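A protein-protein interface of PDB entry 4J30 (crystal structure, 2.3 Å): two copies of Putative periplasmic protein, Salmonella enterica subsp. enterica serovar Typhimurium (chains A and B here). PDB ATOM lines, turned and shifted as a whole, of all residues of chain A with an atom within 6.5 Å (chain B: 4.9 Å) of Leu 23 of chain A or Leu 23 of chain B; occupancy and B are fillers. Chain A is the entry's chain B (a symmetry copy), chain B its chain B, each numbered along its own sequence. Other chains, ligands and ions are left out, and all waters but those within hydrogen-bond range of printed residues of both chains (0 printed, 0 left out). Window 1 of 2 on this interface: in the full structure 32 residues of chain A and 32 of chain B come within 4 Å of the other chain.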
ATOM      1  N   ALA A  18      22.179  31.362  13.708  1.00  0.00           N
ATOM      2  CA  ALA A  18      22.846  31.755  14.946  1.00  0.00           C
ATOM      3  C   ALA A  18      22.030  31.366  16.184  1.00  0.00           C
ATOM      4  O   ALA A  18      22.545  30.715  17.100  1.00  0.00           O
ATOM      5  CB  ALA A  18      23.142  33.274  14.943  1.00  0.00           C
ATOM      6  N   LEU A  19      20.761  31.760  16.204  1.00  0.00           N
ATOM      7  CA  LEU A  19      19.882  31.472  17.344  1.00  0.00           C
ATOM      8  C   LEU A  19      19.703  29.973  17.590  1.00  0.00           C
ATOM      9  O   LEU A  19      19.926  29.482  18.709  1.00  0.00           O
ATOM     10  CB  LEU A  19      18.518  32.155  17.176  1.00  0.00           C
ATOM     11  CG  LEU A  19      17.430  31.807  18.211  1.00  0.00           C
ATOM     12  CD1 LEU A  19      17.890  32.081  19.671  1.00  0.00           C
ATOM     13  CD2 LEU A  19      16.139  32.526  17.905  1.00  0.00           C
ATOM     14  N   SER A  20      19.317  29.244  16.547  1.00  0.00           N
ATOM     15  CA  SER A  20      19.042  27.820  16.692  1.00  0.00           C
ATOM     16  C   SER A  20      20.282  27.017  17.047  1.00  0.00           C
ATOM     17  O   SER A  20      20.219  26.076  17.857  1.00  0.00           O
ATOM     18  CB  SER A  20      18.347  27.251  15.452  1.00  0.00           C
ATOM     19  OG  SER A  20      18.957  27.710  14.276  1.00  0.00           O
ATOM     20  N   HIS A  21      21.410  27.389  16.447  1.00  0.00           N
ATOM     21  CA  HIS A  21      22.674  26.731  16.742  1.00  0.00           C
ATOM     22  C   HIS A  21      23.078  26.975  18.200  1.00  0.00           C
ATOM     23  O   HIS A  21      23.539  26.053  18.883  1.00  0.00           O
ATOM     24  CB  HIS A  21      23.777  27.231  15.809  1.00  0.00           C
ATOM     25  CG  HIS A  21      25.146  26.781  16.211  1.00  0.00           C
ATOM     26  ND1 HIS A  21      25.600  25.500  15.993  1.00  0.00           N
ATOM     27  CD2 HIS A  21      26.155  27.437  16.828  1.00  0.00           C
ATOM     28  CE1 HIS A  21      26.831  25.386  16.454  1.00  0.00           C
ATOM     29  NE2 HIS A  21      27.189  26.547  16.969  1.00  0.00           N
ATOM     30  N   CYS A  22      22.923  28.213  18.661  1.00  0.00           N
ATOM     31  CA  CYS A  22      23.209  28.535  20.062  1.00  0.00           C
ATOM     32  C   CYS A  22      22.336  27.697  20.987  1.00  0.00           C
ATOM     33  O   CYS A  22      22.814  27.180  21.994  1.00  0.00           O
ATOM     34  CB  CYS A  22      23.037  30.027  20.357  1.00  0.00           C
ATOM     35  SG  CYS A  22      23.390  30.501  22.085  1.00  0.00           S
ATOM     36  N   LEU A  23      21.062  27.535  20.638  1.00  0.00           N
ATOM     37  CA  LEU A  23      20.169  26.696  21.453  1.00  0.00           C
ATOM     38  C   LEU A  23      20.628  25.234  21.467  1.00  0.00           C
ATOM     39  O   LEU A  23      20.538  24.553  22.492  1.00  0.00           O
ATOM     40  CB  LEU A  23      18.711  26.832  21.011  1.00  0.00           C
ATOM     41  CG  LEU A  23      18.081  28.221  21.192  1.00  0.00           C
ATOM     42  CD1 LEU A  23      16.762  28.320  20.404  1.00  0.00           C
ATOM     43  CD2 LEU A  23      17.862  28.590  22.691  1.00  0.00           C
ATOM     44  N   ALA A  24      21.134  24.766  20.330  1.00  0.00           N
ATOM     45  CA  ALA A  24      21.758  23.444  20.238  1.00  0.00           C
ATOM     46  C   ALA A  24      22.973  23.293  21.154  1.00  0.00           C
ATOM     47  O   ALA A  24      23.223  22.209  21.674  1.00  0.00           O
ATOM     48  CB  ALA A  24      22.134  23.125  18.784  1.00  0.00           C
ATOM     49  N   LEU A  25      23.720  24.374  21.361  1.00  0.00           N
ATOM     50  CA  LEU A  25      24.867  24.349  22.298  1.00  0.00           C
ATOM     51  C   LEU A  25      24.490  24.296  23.787  1.00  0.00           C
ATOM     52  O   LEU A  25      25.104  23.551  24.554  1.00  0.00           O
ATOM     53  CB  LEU A  25      25.799  25.546  22.073  1.00  0.00           C
ATOM     54  CG  LEU A  25      26.530  25.703  20.739  1.00  0.00           C
ATOM     55  CD1 LEU A  25      27.231  27.063  20.696  1.00  0.00           C
ATOM     56  CD2 LEU A  25      27.535  24.574  20.523  1.00  0.00           C
ATOM     57  N   VAL A  26      23.496  25.075  24.202  1.00  0.00           N
ATOM     58  CA  VAL A  26      23.261  25.278  25.644  1.00  0.00           C
ATOM     59  C   VAL A  26      22.394  24.221  26.330  1.00  0.00           C
ATOM     60  O   VAL A  26      22.561  23.959  27.520  1.00  0.00           O
ATOM     61  CB  VAL A  26      22.703  26.701  25.974  1.00  0.00           C
ATOM     62  CG1 VAL A  26      23.712  27.785  25.586  1.00  0.00           C
ATOM     63  CG2 VAL A  26      21.341  26.940  25.317  1.00  0.00           C
ATOM     64  N   TYR A  27      21.459  23.635  25.591  1.00  0.00           N
ATOM     65  CA  TYR A  27      20.542  22.650  26.164  1.00  0.00           C
ATOM     66  C   TYR A  27      21.194  21.270  26.208  1.00  0.00           C
ATOM     67  O   TYR A  27      21.883  20.886  25.267  1.00  0.00           O
ATOM     68  CB  TYR A  27      19.256  22.585  25.343  1.00  0.00           C
ATOM     69  CG  TYR A  27      18.403  23.844  25.336  1.00  0.00           C
ATOM     70  CD1 TYR A  27      18.212  24.609  26.493  1.00  0.00           C
ATOM     71  CD2 TYR A  27      17.749  24.243  24.172  1.00  0.00           C
ATOM     72  CE1 TYR A  27      17.411  25.748  26.476  1.00  0.00           C
ATOM     73  CE2 TYR A  27      16.942  25.372  24.150  1.00  0.00           C
ATOM     74  CZ  TYR A  27      16.772  26.121  25.296  1.00  0.00           C
ATOM     75  OH  TYR A  27      15.961  27.241  25.243  1.00  0.00           O
ATOM     76  N   LYS A  28      20.975  20.520  27.284  1.00  0.00           N
ATOM     77  CA  LYS A  28      21.599  19.195  27.424  1.00  0.00           C
ATOM     78  C   LYS A  28      20.797  18.048  26.803  1.00  0.00           C
ATOM     79  O   LYS A  28      21.382  17.108  26.254  1.00  0.00           O
ATOM     80  CB  LYS A  28      21.911  18.875  28.894  1.00  0.00           C
ATOM     81  CG  LYS A  28      23.249  19.410  29.394  1.00  0.00           C
ATOM     82  CD  LYS A  28      23.497  18.953  30.834  1.00  0.00           C
ATOM     83  CE  LYS A  28      24.679  19.688  31.470  1.00  0.00           C
ATOM     84  NZ  LYS A  28      24.484  19.863  32.945  1.00  0.00           N
ATOM     85  N   VAL A  32      15.960  17.828  22.337  1.00  0.00           N
ATOM     86  CA  VAL A  32      16.056  19.279  22.149  1.00  0.00           C
ATOM     87  C   VAL A  32      17.287  19.707  21.323  1.00  0.00           C
ATOM     88  O   VAL A  32      17.146  20.499  20.386  1.00  0.00           O
ATOM     89  CB  VAL A  32      16.015  20.053  23.508  1.00  0.00           C
ATOM     90  CG1 VAL A  32      16.217  21.520  23.290  1.00  0.00           C
ATOM     91  CG2 VAL A  32      14.692  19.845  24.204  1.00  0.00           C
ATOM     92  N   LYS A  33      18.475  19.202  21.686  1.00  0.00           N
ATOM     93  CA  LYS A  33      19.714  19.452  20.923  1.00  0.00           C
ATOM     94  C   LYS A  33      19.571  19.033  19.461  1.00  0.00           C
ATOM     95  O   LYS A  33      19.897  19.806  18.568  1.00  0.00           O
ATOM     96  CB  LYS A  33      20.925  18.714  21.518  1.00  0.00           C
ATOM     97  CG  LYS A  33      21.374  19.191  22.896  1.00  0.00           C
ATOM     98  CD  LYS A  33      22.619  18.406  23.383  1.00  0.00           C
ATOM     99  CE  LYS A  33      23.917  19.168  23.120  1.00  0.00           C
ATOM    100  NZ  LYS A  33      23.889  20.539  23.739  1.00  0.00           N
ATOM    101  N   ALA A  36      17.147  21.475  17.614  1.00  0.00           N
ATOM    102  CA  ALA A  36      17.829  22.733  17.317  1.00  0.00           C
ATOM    103  C   ALA A  36      18.900  22.589  16.241  1.00  0.00           C
ATOM    104  O   ALA A  36      19.034  23.470  15.388  1.00  0.00           O
ATOM    105  CB  ALA A  36      18.431  23.327  18.577  1.00  0.00           C
ATOM    106  N   ARG A  37      19.659  21.489  16.296  1.00  0.00           N
ATOM    107  CA  ARG A  37      20.590  21.120  15.228  1.00  0.00           C
ATOM    108  C   ARG A  37      19.912  20.971  13.867  1.00  0.00           C
ATOM    109  O   ARG A  37      20.431  21.440  12.856  1.00  0.00           O
ATOM    110  CB  ARG A  37      21.288  19.797  15.539  1.00  0.00           C
ATOM    111  CG  ARG A  37      22.488  19.895  16.410  1.00  0.00           C
ATOM    112  CD  ARG A  37      23.220  18.564  16.427  1.00  0.00           C
ATOM    113  NE  ARG A  37      24.357  18.580  17.340  1.00  0.00           N
ATOM    114  CZ  ARG A  37      25.398  17.751  17.274  1.00  0.00           C
ATOM    115  NH1 ARG A  37      25.458  16.806  16.339  1.00  0.00           N
ATOM    116  NH2 ARG A  37      26.389  17.863  18.153  1.00  0.00           N
ATOM    117  N   ASN A  78      19.986  29.155  30.507  1.00  0.00           N
ATOM    118  CA  ASN A  78      20.607  28.794  29.239  1.00  0.00           C
ATOM    119  C   ASN A  78      19.970  29.508  28.042  1.00  0.00           C
ATOM    120  O   ASN A  78      20.678  30.043  27.196  1.00  0.00           O
ATOM    121  CB  ASN A  78      20.564  27.283  29.043  1.00  0.00           C
ATOM    122  CG  ASN A  78      21.533  26.557  29.949  1.00  0.00           C
ATOM    123  OD1 ASN A  78      22.673  26.999  30.142  1.00  0.00           O
ATOM    124  ND2 ASN A  78      21.088  25.432  30.514  1.00  0.00           N
ATOM    125  N   THR A  79      18.635  29.516  28.001  1.00  0.00           N
ATOM    126  CA  THR A  79      17.866  30.158  26.941  1.00  0.00           C
ATOM    127  C   THR A  79      18.303  31.611  26.755  1.00  0.00           C
ATOM    128  O   THR A  79      18.407  32.096  25.635  1.00  0.00           O
ATOM    129  CB  THR A  79      16.332  30.116  27.262  1.00  0.00           C
ATOM    130  OG1 THR A  79      15.934  28.786  27.641  1.00  0.00           O
ATOM    131  CG2 THR A  79      15.485  30.603  26.050  1.00  0.00           C
ATOM    132  N   MET A  80      18.571  32.278  27.879  1.00  0.00           N
ATOM    133  CA  MET A  80      18.921  33.693  27.946  1.00  0.00           C
ATOM    134  C   MET A  80      20.294  34.000  27.364  1.00  0.00           C
ATOM    135  O   MET A  80      20.522  35.084  26.833  1.00  0.00           O
ATOM    136  CB  MET A  80      18.875  34.130  29.409  1.00  0.00           C
ATOM    137  CG  MET A  80      19.141  35.587  29.636  1.00  0.00           C
ATOM    138  SD  MET A  80      19.045  36.052  31.508  1.00  0.00           S
ATOM    139  CE  MET A  80      17.111  36.040  31.718  1.00  0.00           C
ATOM    140  N   CYS A  82      21.485  32.598  24.771  1.00  0.00           N
ATOM    141  CA  CYS A  82      21.254  32.642  23.336  1.00  0.00           C
ATOM    142  C   CYS A  82      20.475  33.873  22.876  1.00  0.00           C
ATOM    143  O   CYS A  82      20.689  34.364  21.767  1.00  0.00           O
ATOM    144  CB  CYS A  82      20.583  31.353  22.872  1.00  0.00           C
ATOM    145  SG  CYS A  82      21.659  29.961  23.089  1.00  0.00           S
ATOM    146  N   ILE A  83      19.603  34.380  23.741  1.00  0.00           N
ATOM    147  CA  ILE A  83      18.895  35.633  23.482  1.00  0.00           C
ATOM    148  C   ILE A  83      19.847  36.833  23.570  1.00  0.00           C
ATOM    149  O   ILE A  83      19.812  37.720  22.722  1.00  0.00           O
ATOM    150  CB  ILE A  83      17.674  35.794  24.418  1.00  0.00           C
ATOM    151  CG1 ILE A  83      16.636  34.701  24.078  1.00  0.00           C
ATOM    152  CG2 ILE A  83      17.103  37.228  24.333  1.00  0.00           C
ATOM    153  CD1 ILE A  83      15.410  34.699  24.943  1.00  0.00           C
ATOM    154  N   LEU B  19       9.904  34.944  22.402  1.00  0.00           N
ATOM    155  CA  LEU B  19      10.784  33.850  21.975  1.00  0.00           C
ATOM    156  C   LEU B  19      10.966  32.779  23.053  1.00  0.00           C
ATOM    157  O   LEU B  19      10.745  31.583  22.804  1.00  0.00           O
ATOM    158  CB  LEU B  19      12.147  34.385  21.515  1.00  0.00           C
ATOM    159  CG  LEU B  19      13.237  33.342  21.197  1.00  0.00           C
ATOM    160  CD1 LEU B  19      12.777  32.311  20.126  1.00  0.00           C
ATOM    161  CD2 LEU B  19      14.525  34.010  20.787  1.00  0.00           C
ATOM    162  N   SER B  20      11.352  33.207  24.251  1.00  0.00           N
ATOM    163  CA  SER B  20      11.629  32.263  25.327  1.00  0.00           C
ATOM    164  C   SER B  20      10.391  31.506  25.776  1.00  0.00           C
ATOM    165  O   SER B  20      10.456  30.301  26.072  1.00  0.00           O
ATOM    166  CB  SER B  20      12.324  32.944  26.509  1.00  0.00           C
ATOM    167  OG  SER B  20      11.713  34.167  26.817  1.00  0.00           O
ATOM    168  N   HIS B  21       9.262  32.208  25.821  1.00  0.00           N
ATOM    169  CA  HIS B  21       7.999  31.585  26.187  1.00  0.00           C
ATOM    170  C   HIS B  21       7.596  30.538  25.144  1.00  0.00           C
ATOM    171  O   HIS B  21       7.137  29.447  25.498  1.00  0.00           O
ATOM    172  CB  HIS B  21       6.895  32.633  26.323  1.00  0.00           C
ATOM    173  CG  HIS B  21       5.527  32.042  26.457  1.00  0.00           C
ATOM    174  ND1 HIS B  21       5.074  31.476  27.627  1.00  0.00           N
ATOM    175  CD2 HIS B  21       4.517  31.919  25.565  1.00  0.00           C
ATOM    176  CE1 HIS B  21       3.844  31.033  27.453  1.00  0.00           C
ATOM    177  NE2 HIS B  21       3.484  31.286  26.210  1.00  0.00           N
ATOM    178  N   CYS B  22       7.749  30.881  23.867  1.00  0.00           N
ATOM    179  CA  CYS B  22       7.464  29.927  22.793  1.00  0.00           C
ATOM    180  C   CYS B  22       8.339  28.688  22.937  1.00  0.00           C
ATOM    181  O   CYS B  22       7.863  27.568  22.774  1.00  0.00           O
ATOM    182  CB  CYS B  22       7.634  30.553  21.406  1.00  0.00           C
ATOM    183  SG  CYS B  22       7.282  29.420  20.017  1.00  0.00           S
ATOM    184  N   LEU B  23       9.613  28.880  23.271  1.00  0.00           N
ATOM    185  CA  LEU B  23      10.508  27.731  23.481  1.00  0.00           C
ATOM    186  C   LEU B  23      10.051  26.871  24.664  1.00  0.00           C
ATOM    187  O   LEU B  23      10.143  25.642  24.623  1.00  0.00           O
ATOM    188  CB  LEU B  23      11.965  28.173  23.625  1.00  0.00           C
ATOM    189  CG  LEU B  23      12.593  28.833  22.388  1.00  0.00           C
ATOM    190  CD1 LEU B  23      13.911  29.533  22.764  1.00  0.00           C
ATOM    191  CD2 LEU B  23      12.813  27.826  21.218  1.00  0.00           C
ATOM    192  N   ALA B  24       9.546  27.525  25.705  1.00  0.00           N
ATOM    193  CA  ALA B  24       8.923  26.832  26.835  1.00  0.00           C
ATOM    194  C   ALA B  24       7.709  25.996  26.427  1.00  0.00           C
ATOM    195  O   ALA B  24       7.461  24.943  27.010  1.00  0.00           O
ATOM    196  CB  ALA B  24       8.546  27.830  27.940  1.00  0.00           C
ATOM    197  N   LEU B  25       6.961  26.454  25.427  1.00  0.00           N
ATOM    198  CA  LEU B  25       5.814  25.674  24.905  1.00  0.00           C
ATOM    199  C   LEU B  25       6.193  24.432  24.085  1.00  0.00           C
ATOM    200  O   LEU B  25       5.580  23.374  24.247  1.00  0.00           O
ATOM    201  CB  LEU B  25       4.880  26.552  24.061  1.00  0.00           C
ATOM    202  CG  LEU B  25       4.148  27.727  24.708  1.00  0.00           C
ATOM    203  CD1 LEU B  25       3.445  28.550  23.626  1.00  0.00           C
ATOM    204  CD2 LEU B  25       3.145  27.247  25.754  1.00  0.00           C
ATOM    205  N   VAL B  26       7.186  24.547  23.208  1.00  0.00           N
ATOM    206  CA  VAL B  26       7.422  23.491  22.206  1.00  0.00           C
ATOM    207  C   VAL B  26       8.290  22.320  22.669  1.00  0.00           C
ATOM    208  O   VAL B  26       8.125  21.198  22.192  1.00  0.00           O
ATOM    209  CB  VAL B  26       7.977  24.048  20.855  1.00  0.00           C
ATOM    210  CG1 VAL B  26       6.966  24.992  20.198  1.00  0.00           C
ATOM    211  CG2 VAL B  26       9.339  24.725  21.041  1.00  0.00           C
ATOM    212  N   TYR B  27       9.225  22.583  23.574  1.00  0.00           N
ATOM    213  CA  TYR B  27      10.145  21.547  24.042  1.00  0.00           C
ATOM    214  C   TYR B  27       9.495  20.709  25.142  1.00  0.00           C
ATOM    215  O   TYR B  27       8.806  21.252  26.000  1.00  0.00           O
ATOM    216  CB  TYR B  27      11.430  22.179  24.571  1.00  0.00           C
ATOM    217  CG  TYR B  27      12.281  22.917  23.549  1.00  0.00           C
ATOM    218  CD1 TYR B  27      12.472  22.419  22.255  1.00  0.00           C
ATOM    219  CD2 TYR B  27      12.934  24.097  23.899  1.00  0.00           C
ATOM    220  CE1 TYR B  27      13.271  23.094  21.336  1.00  0.00           C
ATOM    221  CE2 TYR B  27      13.740  24.772  22.991  1.00  0.00           C
ATOM    222  CZ  TYR B  27      13.909  24.273  21.716  1.00  0.00           C
ATOM    223  OH  TYR B  27      14.719  24.968  20.834  1.00  0.00           O
ATOM    224  N   ALA B  36      13.534  27.834  29.957  1.00  0.00           N
ATOM    225  CA  ALA B  36      12.850  28.804  29.106  1.00  0.00           C
ATOM    226  C   ALA B  36      11.780  29.596  29.849  1.00  0.00           C
ATOM    227  O   ALA B  36      11.643  30.801  29.626  1.00  0.00           O
ATOM    228  CB  ALA B  36      12.248  28.122  27.892  1.00  0.00           C
ATOM    229  N   THR B  79      12.042  24.037  17.383  1.00  0.00           N
ATOM    230  CA  THR B  79      12.809  25.273  17.475  1.00  0.00           C
ATOM    231  C   THR B  79      12.370  26.268  16.400  1.00  0.00           C
ATOM    232  O   THR B  79      12.265  27.462  16.655  1.00  0.00           O
ATOM    233  CB  THR B  79      14.344  24.990  17.322  1.00  0.00           C
ATOM    234  OG1 THR B  79      14.744  23.910  18.184  1.00  0.00           O
ATOM    235  CG2 THR B  79      15.190  26.262  17.628  1.00  0.00           C
ATOM    236  N   CYS B  82       9.185  28.452  16.749  1.00  0.00           N
ATOM    237  CA  CYS B  82       9.415  29.646  17.546  1.00  0.00           C
ATOM    238  C   CYS B  82      10.191  30.737  16.809  1.00  0.00           C
ATOM    239  O   CYS B  82       9.976  31.924  17.054  1.00  0.00           O
ATOM    240  CB  CYS B  82      10.087  29.277  18.864  1.00  0.00           C
ATOM    241  SG  CYS B  82       9.013  28.291  19.873  1.00  0.00           S
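Leu 19 of chain B touches its own counterpart, Leu 19 of chain A. Ser 20 of chain A touches Thr 79 of chain B, and with the chains exchanged Thr 79 of chain A touches Ser 20 of chain B. Leu 23 of chain A touches Thr 79 of chain B, and with the chains exchanged Thr 79 of chain A touches Leu 23 of chain B. Ala 36 of chain A touches Thr 79 of chain B, and with the chains exchanged Thr 79 of chain A touches Ala 36 of chain B.
Leu 23 of chain A touches three residues of chain B. Ala 24 of chain A touches none of the printed residues of chain B. Of the printed residues of chain B, Val 32 of chain A touches Tyr 27. Printed residues of chain B within 4 Å of Ala 36 of chain A: Thr 79. Met 80 of chain A touches none of the printed residues of chain B. Of the printed residues of chain A, Leu 19 of chain B touches Leu 19 and Ile 83. Printed residues of chain A within 4 Å of Ser 20 of chain B: Thr 79 and Ile 83. Leu 23 of chain B touches three residues of chain A. Printed residues of chain A within 4 Å of Ala 36 of chain B: Thr 79. The nearest printed residue of chain B that does not touch Leu 23 of chain A is Leu 19 of chain B (5.6 Å).
CD2 of Leu 19 of chain A touches CD2 of Leu 19 of chain B, at 3.6 Å. CD1 of Leu 23 of chain B touches CD1 of Leu 23 of chain A, 3.9 Å away. Tyr 27 of chain B touches Leu 23 of chain A (OH to CD1, 3.9 Å). Leu 23 of chain A touches Thr 79 of chain B. Tyr 27 of chain A touches Leu 23 of chain B. Tyr 27 of chain A touches Tyr 27 of chain B. Val 32 of chain A touches Tyr 27 of chain B. Thr 79 of chain A touches Ser 20 of chain B. CD1 of Leu 23 of chain B touches CG2 of Thr 79 of chain A, 3.8 Å away. Ile 83 of chain A touches Leu 19 of chain B.
Of the 12 printed residues of chain B, 6 touch a printed residue of chain A. Printed residues of chain B that touch a printed residue of chain A: Leu 19, Ser 20, Leu 23, Tyr 27, Ala 36 and Thr 79. Hydrophobic or aromatic side chains of chain B that line the printed part of chain A: Leu 19, Leu 23, Tyr 27 and Ala 36. Hydrophobic or aromatic side chains of chain A within 4 Å of the printed part of chain B: Leu 19, Leu 23, Tyr 27, Val 32, Ala 36 and Ile 83. Among the printed residues, no Asp or Glu carboxylate lies within 4 Å of a Lys or Arg side-chain nitrogen of the other chain.
The backbone NH (N) of Ala 36 of chain A lies close to the side-chain hydroxyl (OG1) of Thr 79 of chain B (3.5 Å). The backbone NH (N) of Ala 36 of chain B lies close to the side-chain hydroxyl (OG1) of Thr 79 of chain A (3.5 Å).
The side-chain sulfur (SG) of Cys 22 of chain A forms a disulfide with the side-chain sulfur (SG) of Cys 82 of chain A. The backbone carbonyl oxygen (O) of Tyr 27 of chain A lies within hydrogen-bond range of the side-chain amino group (NZ) of Lys 33 of chain A (2.5 Å). The side-chain sulfur of Cys 82 of chain B lies within hydrogen-bond range of the backbone NH of Leu 23 of chain B, at 3.5 Å. SG of Cys 22 of chain B forms a disulfide with SG of Cys 82 of chain B (2.1 Å). The side-chain hydroxyl (OG1) of Thr 79 of chain B is in hydrogen-bond range of the side-chain hydroxyl (OH) of Tyr 27 of chain B, 2.9 Å away. OG1 of Thr 79 of chain A sits at hydrogen-bond distance from OH of Tyr 27 of chain A.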
